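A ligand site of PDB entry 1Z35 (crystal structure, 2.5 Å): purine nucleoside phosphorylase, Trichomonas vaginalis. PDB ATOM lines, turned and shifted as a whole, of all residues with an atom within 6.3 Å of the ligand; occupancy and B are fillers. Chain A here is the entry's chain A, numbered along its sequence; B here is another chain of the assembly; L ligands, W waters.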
ATOM      1  N   GLY A  20     -15.021  -8.033   9.049  1.00  0.00           N
ATOM      2  CA  GLY A  20     -15.666  -6.734   8.943  1.00  0.00           C
ATOM      3  C   GLY A  20     -14.813  -5.567   9.414  1.00  0.00           C
ATOM      4  O   GLY A  20     -14.725  -4.543   8.738  1.00  0.00           O
ATOM      5  N   HIS A  62     -14.043  -5.995   5.082  1.00  0.00           N
ATOM      6  CA  HIS A  62     -15.137  -6.035   4.115  1.00  0.00           C
ATOM      7  C   HIS A  62     -16.362  -5.253   4.581  1.00  0.00           C
ATOM      8  O   HIS A  62     -17.410  -5.322   3.943  1.00  0.00           O
ATOM      9  CB  HIS A  62     -15.524  -7.480   3.772  1.00  0.00           C
ATOM     10  CG  HIS A  62     -15.984  -8.289   4.948  1.00  0.00           C
ATOM     11  ND1 HIS A  62     -16.952  -7.842   5.829  1.00  0.00           N
ATOM     12  CD2 HIS A  62     -15.638  -9.530   5.368  1.00  0.00           C
ATOM     13  CE1 HIS A  62     -17.171  -8.778   6.736  1.00  0.00           C
ATOM     14  NE2 HIS A  62     -16.393  -9.809   6.473  1.00  0.00           N
ATOM     15  N   GLY A  63     -16.238  -4.518   5.677  1.00  0.00           N
ATOM     16  CA  GLY A  63     -17.351  -3.740   6.197  1.00  0.00           C
ATOM     17  C   GLY A  63     -18.467  -4.612   6.756  1.00  0.00           C
ATOM     18  O   GLY A  63     -18.332  -5.829   6.820  1.00  0.00           O
ATOM     19  N   MET A  64     -19.576  -4.001   7.140  1.00  0.00           N
ATOM     20  CA  MET A  64     -20.701  -4.743   7.704  1.00  0.00           C
ATOM     21  C   MET A  64     -21.889  -4.793   6.743  1.00  0.00           C
ATOM     22  O   MET A  64     -22.278  -3.764   6.189  1.00  0.00           O
ATOM     23  CB  MET A  64     -21.156  -4.114   9.029  1.00  0.00           C
ATOM     24  CG  MET A  64     -20.045  -3.952  10.056  1.00  0.00           C
ATOM     25  SD  MET A  64     -20.684  -3.346  11.644  1.00  0.00           S
ATOM     26  CE  MET A  64     -20.993  -1.613  11.261  1.00  0.00           C
ATOM     27  N   GLY A  65     -22.464  -5.979   6.566  1.00  0.00           N
ATOM     28  CA  GLY A  65     -23.614  -6.136   5.696  1.00  0.00           C
ATOM     29  C   GLY A  65     -23.358  -6.758   4.332  1.00  0.00           C
ATOM     30  O   GLY A  65     -22.277  -6.619   3.766  1.00  0.00           O
ATOM     31  N   ARG A  87     -14.175 -15.967   5.155  1.00  0.00           N
ATOM     32  CA  ARG A  87     -14.641 -14.941   6.067  1.00  0.00           C
ATOM     33  C   ARG A  87     -14.344 -15.402   7.495  1.00  0.00           C
ATOM     34  O   ARG A  87     -14.705 -16.509   7.893  1.00  0.00           O
ATOM     35  CB  ARG A  87     -16.145 -14.702   5.895  1.00  0.00           C
ATOM     36  CG  ARG A  87     -16.653 -13.493   6.659  1.00  0.00           C
ATOM     37  CD  ARG A  87     -18.166 -13.380   6.622  1.00  0.00           C
ATOM     38  NE  ARG A  87     -18.708 -13.236   7.974  1.00  0.00           N
ATOM     39  CZ  ARG A  87     -18.326 -12.305   8.847  1.00  0.00           C
ATOM     40  NH1 ARG A  87     -17.396 -11.422   8.496  1.00  0.00           N
ATOM     41  NH2 ARG A  87     -18.857 -12.264  10.058  1.00  0.00           N
ATOM     42  N   THR A  90     -16.600 -12.475  14.144  1.00  0.00           N
ATOM     43  CA  THR A  90     -17.433 -12.750  15.309  1.00  0.00           C
ATOM     44  C   THR A  90     -18.883 -12.888  14.873  1.00  0.00           C
ATOM     45  O   THR A  90     -19.228 -12.507  13.760  1.00  0.00           O
ATOM     46  CB  THR A  90     -17.334 -11.612  16.334  1.00  0.00           C
ATOM     47  OG1 THR A  90     -17.725 -10.382  15.704  1.00  0.00           O
ATOM     48  CG2 THR A  90     -15.911 -11.486  16.863  1.00  0.00           C
ATOM     49  N   CYS A  91     -19.712 -13.424  15.759  1.00  0.00           N
ATOM     50  CA  CYS A  91     -21.123 -13.629  15.460  1.00  0.00           C
ATOM     51  C   CYS A  91     -21.928 -13.762  16.744  1.00  0.00           C
ATOM     52  O   CYS A  91     -21.368 -13.937  17.822  1.00  0.00           O
ATOM     53  CB  CYS A  91     -21.299 -14.890  14.623  1.00  0.00           C
ATOM     54  SG  CYS A  91     -20.754 -16.409  15.462  1.00  0.00           S
ATOM     55  N   GLY A  92     -23.251 -13.678  16.609  1.00  0.00           N
ATOM     56  CA  GLY A  92     -24.121 -13.819  17.764  1.00  0.00           C
ATOM     57  C   GLY A  92     -24.764 -15.199  17.767  1.00  0.00           C
ATOM     58  O   GLY A  92     -25.296 -15.633  16.745  1.00  0.00           O
ATOM     59  N   ALA A  93     -24.716 -15.881  18.898  1.00  0.00           N
ATOM     60  CA  ALA A  93     -25.296 -17.206  19.003  1.00  0.00           C
ATOM     61  C   ALA A  93     -26.817 -17.166  18.985  1.00  0.00           C
ATOM     62  O   ALA A  93     -27.427 -16.238  19.519  1.00  0.00           O
ATOM     63  CB  ALA A  93     -24.812 -17.899  20.284  1.00  0.00           C
ATOM     64  N   PHE A 154     -26.957 -17.266   9.883  1.00  0.00           N
ATOM     65  CA  PHE A 154     -27.972 -16.376   9.360  1.00  0.00           C
ATOM     66  C   PHE A 154     -27.325 -15.003   9.188  1.00  0.00           C
ATOM     67  O   PHE A 154     -26.700 -14.494  10.128  1.00  0.00           O
ATOM     68  CB  PHE A 154     -29.157 -16.260  10.319  1.00  0.00           C
ATOM     69  CG  PHE A 154     -30.275 -15.401   9.804  1.00  0.00           C
ATOM     70  CD1 PHE A 154     -31.160 -15.891   8.850  1.00  0.00           C
ATOM     71  CD2 PHE A 154     -30.436 -14.099  10.258  1.00  0.00           C
ATOM     72  CE1 PHE A 154     -32.199 -15.109   8.362  1.00  0.00           C
ATOM     73  CE2 PHE A 154     -31.478 -13.296   9.776  1.00  0.00           C
ATOM     74  CZ  PHE A 154     -32.359 -13.801   8.829  1.00  0.00           C
ATOM     75  N   THR A 156     -28.164 -11.348   8.702  1.00  0.00           N
ATOM     76  CA  THR A 156     -29.249 -10.393   8.802  1.00  0.00           C
ATOM     77  C   THR A 156     -28.878  -9.034   8.227  1.00  0.00           C
ATOM     78  O   THR A 156     -27.703  -8.650   8.219  1.00  0.00           O
ATOM     79  CB  THR A 156     -29.705 -10.206  10.275  1.00  0.00           C
ATOM     80  OG1 THR A 156     -30.878  -9.377  10.317  1.00  0.00           O
ATOM     81  CG2 THR A 156     -28.599  -9.533  11.108  1.00  0.00           C
ATOM     82  N   LEU A 158     -30.575  -6.534   9.409  1.00  0.00           N
ATOM     83  CA  LEU A 158     -30.917  -5.726  10.581  1.00  0.00           C
ATOM     84  C   LEU A 158     -30.290  -6.203  11.882  1.00  0.00           C
ATOM     85  O   LEU A 158     -30.824  -7.105  12.538  1.00  0.00           O
ATOM     86  CB  LEU A 158     -32.453  -5.695  10.763  1.00  0.00           C
ATOM     87  CG  LEU A 158     -33.374  -4.624  10.164  1.00  0.00           C
ATOM     88  CD1 LEU A 158     -32.588  -3.572   9.407  1.00  0.00           C
ATOM     89  CD2 LEU A 158     -34.389  -5.289   9.262  1.00  0.00           C
ATOM     90  N   PHE A 159     -29.169  -5.591  12.274  1.00  0.00           N
ATOM     91  CA  PHE A 159     -28.505  -5.938  13.521  1.00  0.00           C
ATOM     92  C   PHE A 159     -29.543  -5.725  14.641  1.00  0.00           C
ATOM     93  O   PHE A 159     -29.661  -6.546  15.555  1.00  0.00           O
ATOM     94  CB  PHE A 159     -27.303  -5.028  13.755  1.00  0.00           C
ATOM     95  CG  PHE A 159     -26.530  -5.340  15.014  1.00  0.00           C
ATOM     96  CD1 PHE A 159     -25.484  -6.270  14.999  1.00  0.00           C
ATOM     97  CD2 PHE A 159     -26.858  -4.722  16.216  1.00  0.00           C
ATOM     98  CE1 PHE A 159     -24.777  -6.565  16.171  1.00  0.00           C
ATOM     99  CE2 PHE A 159     -26.162  -5.009  17.385  1.00  0.00           C
ATOM    100  CZ  PHE A 159     -25.122  -5.937  17.362  1.00  0.00           C
ATOM    101  N   VAL A 178     -25.572 -15.689  14.139  1.00  0.00           N
ATOM    102  CA  VAL A 178     -25.940 -14.602  13.236  1.00  0.00           C
ATOM    103  C   VAL A 178     -24.774 -13.669  12.957  1.00  0.00           C
ATOM    104  O   VAL A 178     -24.028 -13.300  13.855  1.00  0.00           O
ATOM    105  CB  VAL A 178     -27.059 -13.724  13.844  1.00  0.00           C
ATOM    106  CG1 VAL A 178     -27.466 -12.637  12.844  1.00  0.00           C
ATOM    107  CG2 VAL A 178     -28.239 -14.563  14.215  1.00  0.00           C
ATOM    108  N   GLU A 179     -24.638 -13.298  11.691  1.00  0.00           N
ATOM    109  CA  GLU A 179     -23.622 -12.342  11.275  1.00  0.00           C
ATOM    110  C   GLU A 179     -24.260 -11.536  10.145  1.00  0.00           C
ATOM    111  O   GLU A 179     -25.497 -11.523  10.033  1.00  0.00           O
ATOM    112  CB  GLU A 179     -22.308 -13.032  10.860  1.00  0.00           C
ATOM    113  CG  GLU A 179     -22.427 -14.317  10.052  1.00  0.00           C
ATOM    114  CD  GLU A 179     -22.849 -14.068   8.616  1.00  0.00           C
ATOM    115  OE1 GLU A 179     -24.064 -14.107   8.338  1.00  0.00           O
ATOM    116  OE2 GLU A 179     -21.953 -13.824   7.778  1.00  0.00           O
ATOM    117  N   MET A 180     -23.461 -10.886   9.304  1.00  0.00           N
ATOM    118  CA  MET A 180     -24.063 -10.051   8.266  1.00  0.00           C
ATOM    119  C   MET A 180     -23.415 -10.076   6.881  1.00  0.00           C
ATOM    120  O   MET A 180     -23.527  -9.100   6.145  1.00  0.00           O
ATOM    121  CB  MET A 180     -24.111  -8.595   8.764  1.00  0.00           C
ATOM    122  CG  MET A 180     -24.864  -8.409  10.093  1.00  0.00           C
ATOM    123  SD  MET A 180     -24.840  -6.714  10.772  1.00  0.00           S
ATOM    124  CE  MET A 180     -25.873  -5.842   9.611  1.00  0.00           C
ATOM    125  N   GLU A 181     -22.771 -11.165   6.494  1.00  0.00           N
ATOM    126  CA  GLU A 181     -22.120 -11.191   5.195  1.00  0.00           C
ATOM    127  C   GLU A 181     -22.144 -12.520   4.421  1.00  0.00           C
ATOM    128  O   GLU A 181     -22.295 -12.518   3.203  1.00  0.00           O
ATOM    129  CB  GLU A 181     -20.667 -10.726   5.334  1.00  0.00           C
ATOM    130  CG  GLU A 181     -20.507  -9.289   5.835  1.00  0.00           C
ATOM    131  CD  GLU A 181     -20.688  -9.155   7.343  1.00  0.00           C
ATOM    132  OE1 GLU A 181     -20.863  -8.018   7.827  1.00  0.00           O
ATOM    133  OE2 GLU A 181     -20.643 -10.190   8.043  1.00  0.00           O
ATOM    134  N   CYS A 200     -16.652 -18.310  12.464  1.00  0.00           N
ATOM    135  CA  CYS A 200     -16.789 -17.230  13.429  1.00  0.00           C
ATOM    136  C   CYS A 200     -16.690 -17.689  14.867  1.00  0.00           C
ATOM    137  O   CYS A 200     -16.938 -18.854  15.194  1.00  0.00           O
ATOM    138  CB  CYS A 200     -18.131 -16.510  13.248  1.00  0.00           C
ATOM    139  SG  CYS A 200     -18.364 -15.706  11.658  1.00  0.00           S
ATOM    140  N   SER A 203     -19.294 -14.124  20.020  1.00  0.00           N
ATOM    141  CA  SER A 203     -18.926 -13.099  20.985  1.00  0.00           C
ATOM    142  C   SER A 203     -20.079 -12.710  21.895  1.00  0.00           C
ATOM    143  O   SER A 203     -19.902 -11.901  22.812  1.00  0.00           O
ATOM    144  CB  SER A 203     -18.399 -11.853  20.258  1.00  0.00           C
ATOM    145  OG  SER A 203     -19.407 -11.314  19.410  1.00  0.00           O
ATOM    146  N   ASP A 204     -21.253 -13.279  21.652  1.00  0.00           N
ATOM    147  CA  ASP A 204     -22.425 -12.957  22.462  1.00  0.00           C
ATOM    148  C   ASP A 204     -23.608 -13.857  22.089  1.00  0.00           C
ATOM    149  O   ASP A 204     -23.657 -14.400  20.984  1.00  0.00           O
ATOM    150  CB  ASP A 204     -22.774 -11.476  22.229  1.00  0.00           C
ATOM    151  CG  ASP A 204     -23.894 -10.990  23.131  1.00  0.00           C
ATOM    152  OD1 ASP A 204     -23.771 -11.133  24.369  1.00  0.00           O
ATOM    153  OD2 ASP A 204     -24.875 -10.448  22.606  1.00  0.00           O
ATOM    154  N   ILE A 206     -27.776 -14.061  21.699  1.00  0.00           N
ATOM    155  CA  ILE A 206     -28.942 -13.211  21.575  1.00  0.00           C
ATOM    156  C   ILE A 206     -30.187 -13.670  22.334  1.00  0.00           C
ATOM    157  O   ILE A 206     -31.144 -12.912  22.465  1.00  0.00           O
ATOM    158  CB  ILE A 206     -29.334 -12.990  20.086  1.00  0.00           C
ATOM    159  CG1 ILE A 206     -30.009 -14.235  19.517  1.00  0.00           C
ATOM    160  CG2 ILE A 206     -28.100 -12.646  19.264  1.00  0.00           C
ATOM    161  CD1 ILE A 206     -30.470 -14.068  18.082  1.00  0.00           C
ATOM    162  N   PRO B   3     -21.851  -1.673  20.736  1.00  0.00           N
ATOM    163  CA  PRO B   3     -20.951  -2.619  20.080  1.00  0.00           C
ATOM    164  C   PRO B   3     -20.085  -1.996  18.980  1.00  0.00           C
ATOM    165  O   PRO B   3     -19.051  -2.564  18.622  1.00  0.00           O
ATOM    166  CB  PRO B   3     -21.910  -3.664  19.510  1.00  0.00           C
ATOM    167  CG  PRO B   3     -23.036  -3.650  20.494  1.00  0.00           C
ATOM    168  CD  PRO B   3     -23.239  -2.171  20.707  1.00  0.00           C
ATOM    169  N   HIS B   4     -20.506  -0.851  18.446  1.00  0.00           N
ATOM    170  CA  HIS B   4     -19.759  -0.207  17.364  1.00  0.00           C
ATOM    171  C   HIS B   4     -19.307   1.209  17.690  1.00  0.00           C
ATOM    172  O   HIS B   4     -18.782   1.911  16.814  1.00  0.00           O
ATOM    173  CB  HIS B   4     -20.600  -0.165  16.094  1.00  0.00           C
ATOM    174  CG  HIS B   4     -21.401  -1.418  15.860  1.00  0.00           C
ATOM    175  ND1 HIS B   4     -22.602  -1.654  16.474  1.00  0.00           N
ATOM    176  CD2 HIS B   4     -21.141  -2.519  15.102  1.00  0.00           C
ATOM    177  CE1 HIS B   4     -23.057  -2.846  16.116  1.00  0.00           C
ATOM    178  NE2 HIS B   4     -22.180  -3.387  15.286  1.00  0.00           N
ATOM    179  N   ARG B  43     -13.668  -0.081  14.756  1.00  0.00           N
ATOM    180  CA  ARG B  43     -13.724  -0.482  13.353  1.00  0.00           C
ATOM    181  C   ARG B  43     -13.204   0.630  12.454  1.00  0.00           C
ATOM    182  O   ARG B  43     -13.602   0.736  11.291  1.00  0.00           O
ATOM    183  CB  ARG B  43     -15.153  -0.847  12.949  1.00  0.00           C
ATOM    184  CG  ARG B  43     -15.685  -2.084  13.655  1.00  0.00           C
ATOM    185  CD  ARG B  43     -17.180  -2.283  13.408  1.00  0.00           C
ATOM    186  NE  ARG B  43     -17.635  -3.522  14.031  1.00  0.00           N
ATOM    187  CZ  ARG B  43     -17.552  -4.718  13.466  1.00  0.00           C
ATOM    188  NH1 ARG B  43     -17.050  -4.846  12.236  1.00  0.00           N
ATOM    189  NH2 ARG B  43     -17.961  -5.786  14.124  1.00  0.00           N
ATOM    190  N   ILE B  71     -27.058   0.469  11.367  1.00  0.00           N
ATOM    191  CA  ILE B  71     -26.459   0.197  12.664  1.00  0.00           C
ATOM    192  C   ILE B  71     -26.012   1.504  13.329  1.00  0.00           C
ATOM    193  O   ILE B  71     -26.393   1.806  14.461  1.00  0.00           O
ATOM    194  CB  ILE B  71     -25.226  -0.722  12.509  1.00  0.00           C
ATOM    195  CG1 ILE B  71     -25.678  -2.149  12.219  1.00  0.00           C
ATOM    196  CG2 ILE B  71     -24.363  -0.664  13.755  1.00  0.00           C
ATOM    197  CD1 ILE B  71     -24.538  -3.106  11.911  1.00  0.00           C
HETATM  198  O1  LIG L   1     -21.858  -5.893  14.638  1.00  0.00           O
HETATM  199  C1  LIG L   1     -22.229  -6.505  13.385  1.00  0.00           C
HETATM  200  C2  LIG L   1     -21.006  -6.985  12.595  1.00  0.00           C
HETATM  201  O2  LIG L   1     -20.172  -7.955  13.305  1.00  0.00           O
HETATM  202  C3  LIG L   1     -20.584  -9.295  13.026  1.00  0.00           C
HETATM  203  N1  LIG L   1     -21.397  -9.713  14.238  1.00  0.00           N
HETATM  204  C4  LIG L   1     -22.792  -9.817  14.452  1.00  0.00           C
HETATM  205  N2  LIG L   1     -23.839  -9.547  13.559  1.00  0.00           N
HETATM  206  C5  LIG L   1     -25.067  -9.738  14.101  1.00  0.00           C
HETATM  207  F1  LIG L   1     -26.125  -9.510  13.359  1.00  0.00           F
HETATM  208  N3  LIG L   1     -25.335 -10.143  15.371  1.00  0.00           N
HETATM  209  C6  LIG L   1     -24.281 -10.395  16.225  1.00  0.00           C
HETATM  210  N4  LIG L   1     -24.538 -10.790  17.450  1.00  0.00           N
HETATM  211  C7  LIG L   1     -22.938 -10.241  15.766  1.00  0.00           C
HETATM  212  N5  LIG L   1     -21.710 -10.412  16.364  1.00  0.00           N
HETATM  213  C8  LIG L   1     -20.868 -10.087  15.417  1.00  0.00           C
HETATM  214  C9  LIG L   1     -21.338  -9.210  11.634  1.00  0.00           C
HETATM  215  O3  LIG L   1     -20.791 -10.106  10.608  1.00  0.00           O
HETATM  216  C10 LIG L   1     -21.327  -7.680  11.250  1.00  0.00           C
HETATM  217  O4  LIG L   1     -20.288  -7.376  10.340  1.00  0.00           O
HETATM  218  O   HOH W   1     -19.905  -6.742  16.806  1.00  0.00           O
HETATM  219  O   HOH W   2     -17.653  -7.349  11.163  1.00  0.00           O
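Water W2 lies within hydrogen-bond range of O4 of the ligand (2.8 Å), NH1 of Arg 43 of chain B (2.8 Å) and N of Gly 20 (3.4 Å). Water W1 bridges an oxygen (O1) of the ligand (3.0 Å) and the guanidinium group of Arg 43 of chain B (3.4 Å).
The guanidinium group of Arg 87 sits at hydrogen-bond distance from an oxygen (O3) of the ligand (2.9 Å). N of Met 180 is in hydrogen-bond range of O3 of the ligand. NH2 of Arg 43 of chain B is in hydrogen-bond range of O2 of the ligand (3.2 Å). A ring nitrogen (NE2) of His 4 of chain B is in hydrogen-bond range of an oxygen (O1) of the ligand. An oxygen (O3) of the ligand lies within hydrogen-bond range of the side-chain carboxylate (OE2) of Glu 181 (2.6 Å).
The backbone NH of Gly 92 sits close to a nitrogen (N4) of the ligand (3.3 Å). Met 64 touches the ligand (CG to O4, 3.4 Å). OG1 of Thr 90 touches C8 of the ligand (3.2 Å). Cys 91 touches the ligand. CG2 of Thr 156 touches F1 of the ligand (3.3 Å). Phe 159 touches the ligand (CE1 to O1, 3.4 Å). Val 178 touches the ligand (CG1 to F1, 3.4 Å). Glu 179 touches the ligand. Ser 203 touches the ligand. Hydrophobic or aromatic side chains within 4 Å of the ligand: Met 64, Phe 159, Val 178, Met 180 and His 4 of chain B. Within 4 Å of the ligand: Met 64, Arg 87, Thr 90, Cys 91, Gly 92, Thr 156, Phe 159, Val 178, Glu 179, Met 180, Glu 181, Ser 203, His 4 of chain B and Arg 43 of chain B.
The backbone NH of Thr 156 is in hydrogen-bond range of the backbone carbonyl oxygen of Glu 179 (3.0 Å). N of Val 178 lies within hydrogen-bond range of O of Gly 92. O of Cys 91 is in hydrogen-bond range of N of Ser 203 (3.0 Å). The guanidinium group (NH1) of Arg 87 sits at hydrogen-bond distance from a ring nitrogen (NE2) of His 62 (2.8 Å). OG1 of Thr 156 sits at hydrogen-bond distance from N of Leu 158, 3.0 Å away. The backbone NH of Glu 179 sits at hydrogen-bond distance from the backbone carbonyl oxygen of Phe 154 (2.9 Å). OE2 of Glu 181 lies within salt-bridge range of NH2 of Arg 87 (3.4 Å). The backbone NH of Glu 181 is in hydrogen-bond range of the side-chain carboxylate of Glu 179.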
